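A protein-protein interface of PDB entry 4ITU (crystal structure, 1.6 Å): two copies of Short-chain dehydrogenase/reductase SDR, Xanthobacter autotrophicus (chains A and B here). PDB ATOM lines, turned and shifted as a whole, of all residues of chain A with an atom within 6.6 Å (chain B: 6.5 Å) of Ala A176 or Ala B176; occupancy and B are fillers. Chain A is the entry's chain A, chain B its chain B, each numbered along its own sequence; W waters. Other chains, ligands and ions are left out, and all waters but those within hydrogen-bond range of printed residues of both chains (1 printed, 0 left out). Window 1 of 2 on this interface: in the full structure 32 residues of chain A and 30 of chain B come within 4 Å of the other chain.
Of the 14 printed residues of chain A, 7 touch a printed residue of chain B. Printed residues of chain A that touch a printed residue of chain B: Met A126, Gly A160, Cys A171, Ala A172, Gly A175, Ala A176 and Asn A179. Hydrophobic or aromatic side chains of chain B within 4 Å of the printed part of chain A: Met B126 and Ala B176. Along chain B the printed residues that touch a printed residue of chain A span positions 126 to 179.
Met A126 touches its own counterpart, Met B126. Gly A160 touches Asn B179, and with the chains exchanged Asn A179 touches Gly B160. Cys A171 touches Asn B179, and with the chains exchanged Asn A179 touches Cys B171. Ala B176 touches its own counterpart, Ala A176. 14 positions are printed for both chains. Of the 13 pairs that touch across the chains among the printed residues, 13 have their exchanged pair printed and touching as well.
The side-chain sulfur (SD) of Met A126 sits at hydrogen-bond distance from the backbone NH (N) of Ala A173 (3.6 Å). The backbone NH (N) of Ala B173 sits at hydrogen-bond distance from the side-chain sulfur (SD) of Met B126.
Printed residues of chain B within 4 Å of Met A126: Met B126 (3.3 Å). Of chain B, only Ala B172, Gly B175 and Ala B176 come within 4 Å of Ala A176. Printed residues of chain A within 4 Å of Gly B160: Asn A179 (3.3 Å). Of the printed residues of chain A, Gly B175 touches Gly A175, Ala A176 and Asn A179. Of chain A, only Ala A172, Gly A175 and Ala A176 come within 4 Å of Ala B176. The nearest residue of chain A that does not touch Ala B176 is Met A126 (4.7 Å).
Among the printed residues, merely in contact across the chains: Ala A172 with Ala B176 (3.2 Å), Ala A176 with Ala B172 (3.2 Å), Met A126 with Met B126 (3.3 Å), Asn A179 with Gly B160 (3.3 Å), Gly A160 with Asn B179 (3.4 Å), Gly A175 with Gly B175 (3.6 Å), Ala A176 with Ala B176 (3.7 Å), Gly A175 with Asn B179 (3.9 Å), Asn A179 with Gly B175 (3.9 Å), Gly A175 with Ala B176 (3.9 Å) and Ala A176 with Gly B175 (3.9 Å).
Water W1 lies within hydrogen-bond range of the backbone carbonyl oxygen of Gly A175 (2.8 Å) and the backbone carbonyl oxygen of Gly B175 (2.8 Å).
The backbone carbonyl oxygen (O) of Cys A171 lies within hydrogen-bond range of the side-chain amide nitrogen (ND2) of Asn B179 (3.1 Å). O of Cys B171 is in hydrogen-bond range of ND2 of Asn A179, 3.1 Å away.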
ATOM      1  N   MET A 126      -4.499  -5.865  13.821  1.00  0.00           N
ATOM      2  CA  MET A 126      -3.714  -7.099  13.928  1.00  0.00           C
ATOM      3  C   MET A 126      -2.402  -6.991  13.147  1.00  0.00           C
ATOM      4  O   MET A 126      -1.364  -7.486  13.588  1.00  0.00           O
ATOM      5  CB  MET A 126      -4.524  -8.310  13.453  1.00  0.00           C
ATOM      6  CG  MET A 126      -5.739  -8.607  14.327  1.00  0.00           C
ATOM      7  SD  MET A 126      -5.273  -9.245  15.955  1.00  0.00           S
ATOM      8  CE  MET A 126      -4.405 -10.689  15.486  1.00  0.00           C
ATOM      9  N   VAL A 130       0.701  -7.310  15.517  1.00  0.00           N
ATOM     10  CA  VAL A 130       1.222  -8.664  15.486  1.00  0.00           C
ATOM     11  C   VAL A 130       2.161  -8.888  14.309  1.00  0.00           C
ATOM     12  O   VAL A 130       3.298  -9.302  14.499  1.00  0.00           O
ATOM     13  CB  VAL A 130       0.106  -9.727  15.498  1.00  0.00           C
ATOM     14  CG1 VAL A 130       0.730 -11.107  15.656  1.00  0.00           C
ATOM     15  CG2 VAL A 130      -0.894  -9.460  16.642  1.00  0.00           C
ATOM     16  N   GLY A 160      -3.509  -6.848  26.751  1.00  0.00           N
ATOM     17  CA  GLY A 160      -3.079  -8.154  26.291  1.00  0.00           C
ATOM     18  C   GLY A 160      -3.211  -9.216  27.365  1.00  0.00           C
ATOM     19  O   GLY A 160      -2.992 -10.397  27.092  1.00  0.00           O
ATOM     20  N   CYS A 171      -7.402  -6.140  21.915  1.00  0.00           N
ATOM     21  CA  CYS A 171      -7.155  -7.167  22.930  1.00  0.00           C
ATOM     22  C   CYS A 171      -6.636  -8.462  22.314  1.00  0.00           C
ATOM     23  O   CYS A 171      -5.778  -9.137  22.896  1.00  0.00           O
ATOM     24  CB  CYS A 171      -8.405  -7.427  23.768  1.00  0.00           C
ATOM     25  SG  CYS A 171      -8.771  -6.086  24.924  1.00  0.00           S
ATOM     26  N   ALA A 172      -7.140  -8.813  21.132  1.00  0.00           N
ATOM     27  CA  ALA A 172      -6.621  -9.962  20.399  1.00  0.00           C
ATOM     28  C   ALA A 172      -5.162  -9.746  20.007  1.00  0.00           C
ATOM     29  O   ALA A 172      -4.318 -10.629  20.204  1.00  0.00           O
ATOM     30  CB  ALA A 172      -7.460 -10.230  19.165  1.00  0.00           C
ATOM     31  N   ALA A 173      -4.855  -8.574  19.464  1.00  0.00           N
ATOM     32  CA  ALA A 173      -3.501  -8.285  18.995  1.00  0.00           C
ATOM     33  C   ALA A 173      -2.508  -8.301  20.147  1.00  0.00           C
ATOM     34  O   ALA A 173      -1.446  -8.913  20.053  1.00  0.00           O
ATOM     35  CB  ALA A 173      -3.467  -6.953  18.284  1.00  0.00           C
ATOM     36  N   LYS A 174      -2.850  -7.650  21.247  1.00  0.00           N
ATOM     37  CA  LYS A 174      -1.929  -7.588  22.377  1.00  0.00           C
ATOM     38  C   LYS A 174      -1.800  -8.962  23.046  1.00  0.00           C
ATOM     39  O   LYS A 174      -0.726  -9.315  23.528  1.00  0.00           O
ATOM     40  CB  LYS A 174      -2.337  -6.476  23.344  1.00  0.00           C
ATOM     41  CG  LYS A 174      -2.197  -5.061  22.735  1.00  0.00           C
ATOM     42  CD  LYS A 174      -0.803  -4.898  22.088  1.00  0.00           C
ATOM     43  CE  LYS A 174      -0.457  -3.447  21.812  1.00  0.00           C
ATOM     44  NZ  LYS A 174       0.913  -3.275  21.227  1.00  0.00           N
ATOM     45  N   GLY A 175      -2.878  -9.746  23.049  1.00  0.00           N
ATOM     46  CA  GLY A 175      -2.837 -11.113  23.553  1.00  0.00           C
ATOM     47  C   GLY A 175      -1.893 -11.966  22.720  1.00  0.00           C
ATOM     48  O   GLY A 175      -1.144 -12.797  23.250  1.00  0.00           O
ATOM     49  N   ALA A 176      -1.918 -11.758  21.404  1.00  0.00           N
ATOM     50  CA  ALA A 176      -0.997 -12.453  20.511  1.00  0.00           C
ATOM     51  C   ALA A 176       0.445 -12.093  20.836  1.00  0.00           C
ATOM     52  O   ALA A 176       1.314 -12.968  20.898  1.00  0.00           O
ATOM     53  CB  ALA A 176      -1.332 -12.120  19.067  1.00  0.00           C
ATOM     54  N   ILE A 177       0.700 -10.810  21.063  1.00  0.00           N
ATOM     55  CA  ILE A 177       2.059 -10.357  21.353  1.00  0.00           C
ATOM     56  C   ILE A 177       2.583 -10.944  22.665  1.00  0.00           C
ATOM     57  O   ILE A 177       3.733 -11.403  22.725  1.00  0.00           O
ATOM     58  CB  ILE A 177       2.168  -8.831  21.352  1.00  0.00           C
ATOM     59  CG1 ILE A 177       2.000  -8.290  19.932  1.00  0.00           C
ATOM     60  CG2 ILE A 177       3.521  -8.385  21.907  1.00  0.00           C
ATOM     61  CD1 ILE A 177       1.768  -6.769  19.878  1.00  0.00           C
ATOM     62  N   VAL A 178       1.748 -10.980  23.700  1.00  0.00           N
ATOM     63  CA  VAL A 178       2.185 -11.550  24.972  1.00  0.00           C
ATOM     64  C   VAL A 178       2.642 -12.999  24.790  1.00  0.00           C
ATOM     65  O   VAL A 178       3.743 -13.374  25.215  1.00  0.00           O
ATOM     66  CB  VAL A 178       1.104 -11.459  26.061  1.00  0.00           C
ATOM     67  CG1 VAL A 178       1.566 -12.201  27.313  1.00  0.00           C
ATOM     68  CG2 VAL A 178       0.811  -9.996  26.403  1.00  0.00           C
ATOM     69  N   ASN A 179       1.838 -13.819  24.123  1.00  0.00           N
ATOM     70  CA  ASN A 179       2.256 -15.207  23.973  1.00  0.00           C
ATOM     71  C   ASN A 179       3.304 -15.425  22.887  1.00  0.00           C
ATOM     72  O   ASN A 179       4.115 -16.348  23.004  1.00  0.00           O
ATOM     73  CB  ASN A 179       1.084 -16.165  23.813  1.00  0.00           C
ATOM     74  CG  ASN A 179       1.452 -17.566  24.218  1.00  0.00           C
ATOM     75  OD1 ASN A 179       1.959 -17.786  25.330  1.00  0.00           O
ATOM     76  ND2 ASN A 179       1.263 -18.517  23.313  1.00  0.00           N
ATOM     77  N   LEU A 180       3.318 -14.585  21.848  1.00  0.00           N
ATOM     78  CA  LEU A 180       4.393 -14.650  20.846  1.00  0.00           C
ATOM     79  C   LEU A 180       5.745 -14.411  21.506  1.00  0.00           C
ATOM     80  O   LEU A 180       6.755 -15.036  21.149  1.00  0.00           O
ATOM     81  CB  LEU A 180       4.161 -13.632  19.729  1.00  0.00           C
ATOM     82  CG  LEU A 180       5.264 -13.542  18.672  1.00  0.00           C
ATOM     83  CD1 LEU A 180       5.525 -14.909  18.029  1.00  0.00           C
ATOM     84  CD2 LEU A 180       4.867 -12.496  17.626  1.00  0.00           C
ATOM     85  N   THR A 181       5.757 -13.512  22.480  1.00  0.00           N
ATOM     86  CA  THR A 181       6.962 -13.229  23.250  1.00  0.00           C
ATOM     87  C   THR A 181       7.474 -14.485  23.959  1.00  0.00           C
ATOM     88  O   THR A 181       8.670 -14.775  23.924  1.00  0.00           O
ATOM     89  CB  THR A 181       6.687 -12.119  24.257  1.00  0.00           C
ATOM     90  OG1 THR A 181       6.346 -10.928  23.530  1.00  0.00           O
ATOM     91  CG2 THR A 181       7.913 -11.857  25.121  1.00  0.00           C
ATOM     92  N   MET B 126      -3.161 -17.140  11.408  1.00  0.00           N
ATOM     93  CA  MET B 126      -3.861 -16.076  12.127  1.00  0.00           C
ATOM     94  C   MET B 126      -5.306 -15.933  11.629  1.00  0.00           C
ATOM     95  O   MET B 126      -6.234 -15.784  12.429  1.00  0.00           O
ATOM     96  CB  MET B 126      -3.120 -14.752  11.987  1.00  0.00           C
ATOM     97  CG  MET B 126      -1.739 -14.736  12.626  1.00  0.00           C
ATOM     98  SD  MET B 126      -1.778 -14.869  14.436  1.00  0.00           S
ATOM     99  CE  MET B 126      -2.722 -13.442  14.811  1.00  0.00           C
ATOM    100  N   VAL B 130      -7.853 -16.756  14.481  1.00  0.00           N
ATOM    101  CA  VAL B 130      -8.326 -15.521  15.090  1.00  0.00           C
ATOM    102  C   VAL B 130      -9.449 -14.863  14.295  1.00  0.00           C
ATOM    103  O   VAL B 130     -10.507 -14.574  14.839  1.00  0.00           O
ATOM    104  CB  VAL B 130      -7.181 -14.513  15.321  1.00  0.00           C
ATOM    105  CG1 VAL B 130      -7.685 -13.328  16.152  1.00  0.00           C
ATOM    106  CG2 VAL B 130      -5.982 -15.192  16.006  1.00  0.00           C
ATOM    107  N   GLY B 160      -1.409 -21.355  23.553  1.00  0.00           N
ATOM    108  CA  GLY B 160      -1.858 -19.989  23.703  1.00  0.00           C
ATOM    109  C   GLY B 160      -1.491 -19.442  25.068  1.00  0.00           C
ATOM    110  O   GLY B 160      -1.635 -18.236  25.315  1.00  0.00           O
ATOM    111  N   CYS B 171       1.300 -19.943  18.125  1.00  0.00           N
ATOM    112  CA  CYS B 171       1.307 -19.410  19.494  1.00  0.00           C
ATOM    113  C   CYS B 171       0.763 -17.995  19.556  1.00  0.00           C
ATOM    114  O   CYS B 171       0.101 -17.622  20.537  1.00  0.00           O
ATOM    115  CB  CYS B 171       2.710 -19.447  20.092  1.00  0.00           C
ATOM    116  SG  CYS B 171       3.264 -21.097  20.528  1.00  0.00           S
ATOM    117  N   ALA B 172       1.065 -17.187  18.538  1.00  0.00           N
ATOM    118  CA  ALA B 172       0.462 -15.860  18.424  1.00  0.00           C
ATOM    119  C   ALA B 172      -1.054 -15.989  18.308  1.00  0.00           C
ATOM    120  O   ALA B 172      -1.797 -15.325  19.044  1.00  0.00           O
ATOM    121  CB  ALA B 172       1.010 -15.129  17.217  1.00  0.00           C
ATOM    122  N   ALA B 173      -1.511 -16.846  17.395  1.00  0.00           N
ATOM    123  CA  ALA B 173      -2.945 -17.014  17.133  1.00  0.00           C
ATOM    124  C   ALA B 173      -3.691 -17.486  18.374  1.00  0.00           C
ATOM    125  O   ALA B 173      -4.719 -16.911  18.747  1.00  0.00           O
ATOM    126  CB  ALA B 173      -3.172 -17.974  15.996  1.00  0.00           C
ATOM    127  N   LYS B 174      -3.183 -18.526  19.023  1.00  0.00           N
ATOM    128  CA  LYS B 174      -3.876 -19.044  20.196  1.00  0.00           C
ATOM    129  C   LYS B 174      -3.794 -18.056  21.366  1.00  0.00           C
ATOM    130  O   LYS B 174      -4.724 -17.956  22.163  1.00  0.00           O
ATOM    131  CB  LYS B 174      -3.374 -20.441  20.575  1.00  0.00           C
ATOM    132  CG  LYS B 174      -3.702 -21.519  19.525  1.00  0.00           C
ATOM    133  CD  LYS B 174      -5.196 -21.448  19.119  1.00  0.00           C
ATOM    134  CE  LYS B 174      -5.685 -22.738  18.468  1.00  0.00           C
ATOM    135  NZ  LYS B 174      -7.121 -22.644  18.063  1.00  0.00           N
ATOM    136  N   GLY B 175      -2.705 -17.300  21.463  1.00  0.00           N
ATOM    137  CA  GLY B 175      -2.604 -16.259  22.476  1.00  0.00           C
ATOM    138  C   GLY B 175      -3.665 -15.194  22.251  1.00  0.00           C
ATOM    139  O   GLY B 175      -4.282 -14.676  23.196  1.00  0.00           O
ATOM    140  N   ALA B 176      -3.891 -14.866  20.985  1.00  0.00           N
ATOM    141  CA  ALA B 176      -4.919 -13.909  20.630  1.00  0.00           C
ATOM    142  C   ALA B 176      -6.291 -14.416  21.056  1.00  0.00           C
ATOM    143  O   ALA B 176      -7.077 -13.660  21.634  1.00  0.00           O
ATOM    144  CB  ALA B 176      -4.887 -13.595  19.139  1.00  0.00           C
ATOM    145  N   ILE B 177      -6.567 -15.696  20.811  1.00  0.00           N
ATOM    146  CA  ILE B 177      -7.877 -16.266  21.141  1.00  0.00           C
ATOM    147  C   ILE B 177      -8.126 -16.262  22.645  1.00  0.00           C
ATOM    148  O   ILE B 177      -9.228 -15.921  23.091  1.00  0.00           O
ATOM    149  CB  ILE B 177      -8.046 -17.678  20.553  1.00  0.00           C
ATOM    150  CG1 ILE B 177      -8.221 -17.589  19.037  1.00  0.00           C
ATOM    151  CG2 ILE B 177      -9.243 -18.385  21.191  1.00  0.00           C
ATOM    152  CD1 ILE B 177      -8.065 -18.935  18.345  1.00  0.00           C
ATOM    153  N   VAL B 178      -7.097 -16.586  23.425  1.00  0.00           N
ATOM    154  CA  VAL B 178      -7.222 -16.587  24.881  1.00  0.00           C
ATOM    155  C   VAL B 178      -7.633 -15.202  25.372  1.00  0.00           C
ATOM    156  O   VAL B 178      -8.619 -15.067  26.110  1.00  0.00           O
ATOM    157  CB  VAL B 178      -5.932 -17.065  25.571  1.00  0.00           C
ATOM    158  CG1 VAL B 178      -5.987 -16.794  27.076  1.00  0.00           C
ATOM    159  CG2 VAL B 178      -5.708 -18.561  25.307  1.00  0.00           C
ATOM    160  N   ASN B 179      -6.934 -14.160  24.934  1.00  0.00           N
ATOM    161  CA  ASN B 179      -7.312 -12.834  25.418  1.00  0.00           C
ATOM    162  C   ASN B 179      -8.560 -12.263  24.763  1.00  0.00           C
ATOM    163  O   ASN B 179      -9.296 -11.522  25.410  1.00  0.00           O
ATOM    164  CB  ASN B 179      -6.165 -11.823  25.387  1.00  0.00           C
ATOM    165  CG  ASN B 179      -6.360 -10.722  26.410  1.00  0.00           C
ATOM    166  OD1 ASN B 179      -6.591 -10.997  27.592  1.00  0.00           O
ATOM    167  ND2 ASN B 179      -6.300  -9.468  25.965  1.00  0.00           N
ATOM    168  N   LEU B 180      -8.812 -12.605  23.498  1.00  0.00           N
ATOM    169  CA  LEU B 180     -10.054 -12.193  22.852  1.00  0.00           C
ATOM    170  C   LEU B 180     -11.248 -12.724  23.640  1.00  0.00           C
ATOM    171  O   LEU B 180     -12.267 -12.049  23.784  1.00  0.00           O
ATOM    172  CB  LEU B 180     -10.115 -12.689  21.413  1.00  0.00           C
ATOM    173  CG  LEU B 180     -11.405 -12.394  20.664  1.00  0.00           C
ATOM    174  CD1 LEU B 180     -11.706 -10.876  20.656  1.00  0.00           C
ATOM    175  CD2 LEU B 180     -11.296 -12.941  19.238  1.00  0.00           C
ATOM    176  N   THR B 181     -11.102 -13.939  24.154  1.00  0.00           N
ATOM    177  CA  THR B 181     -12.143 -14.567  24.967  1.00  0.00           C
ATOM    178  C   THR B 181     -12.457 -13.710  26.199  1.00  0.00           C
ATOM    179  O   THR B 181     -13.626 -13.481  26.521  1.00  0.00           O
ATOM    180  CB  THR B 181     -11.725 -15.977  25.414  1.00  0.00           C
ATOM    181  OG1 THR B 181     -11.570 -16.821  24.254  1.00  0.00           O
ATOM    182  CG2 THR B 181     -12.778 -16.571  26.367  1.00  0.00           C
HETATM  183  O   HOH W   1      -2.507 -14.132  25.252  1.00  0.00           O
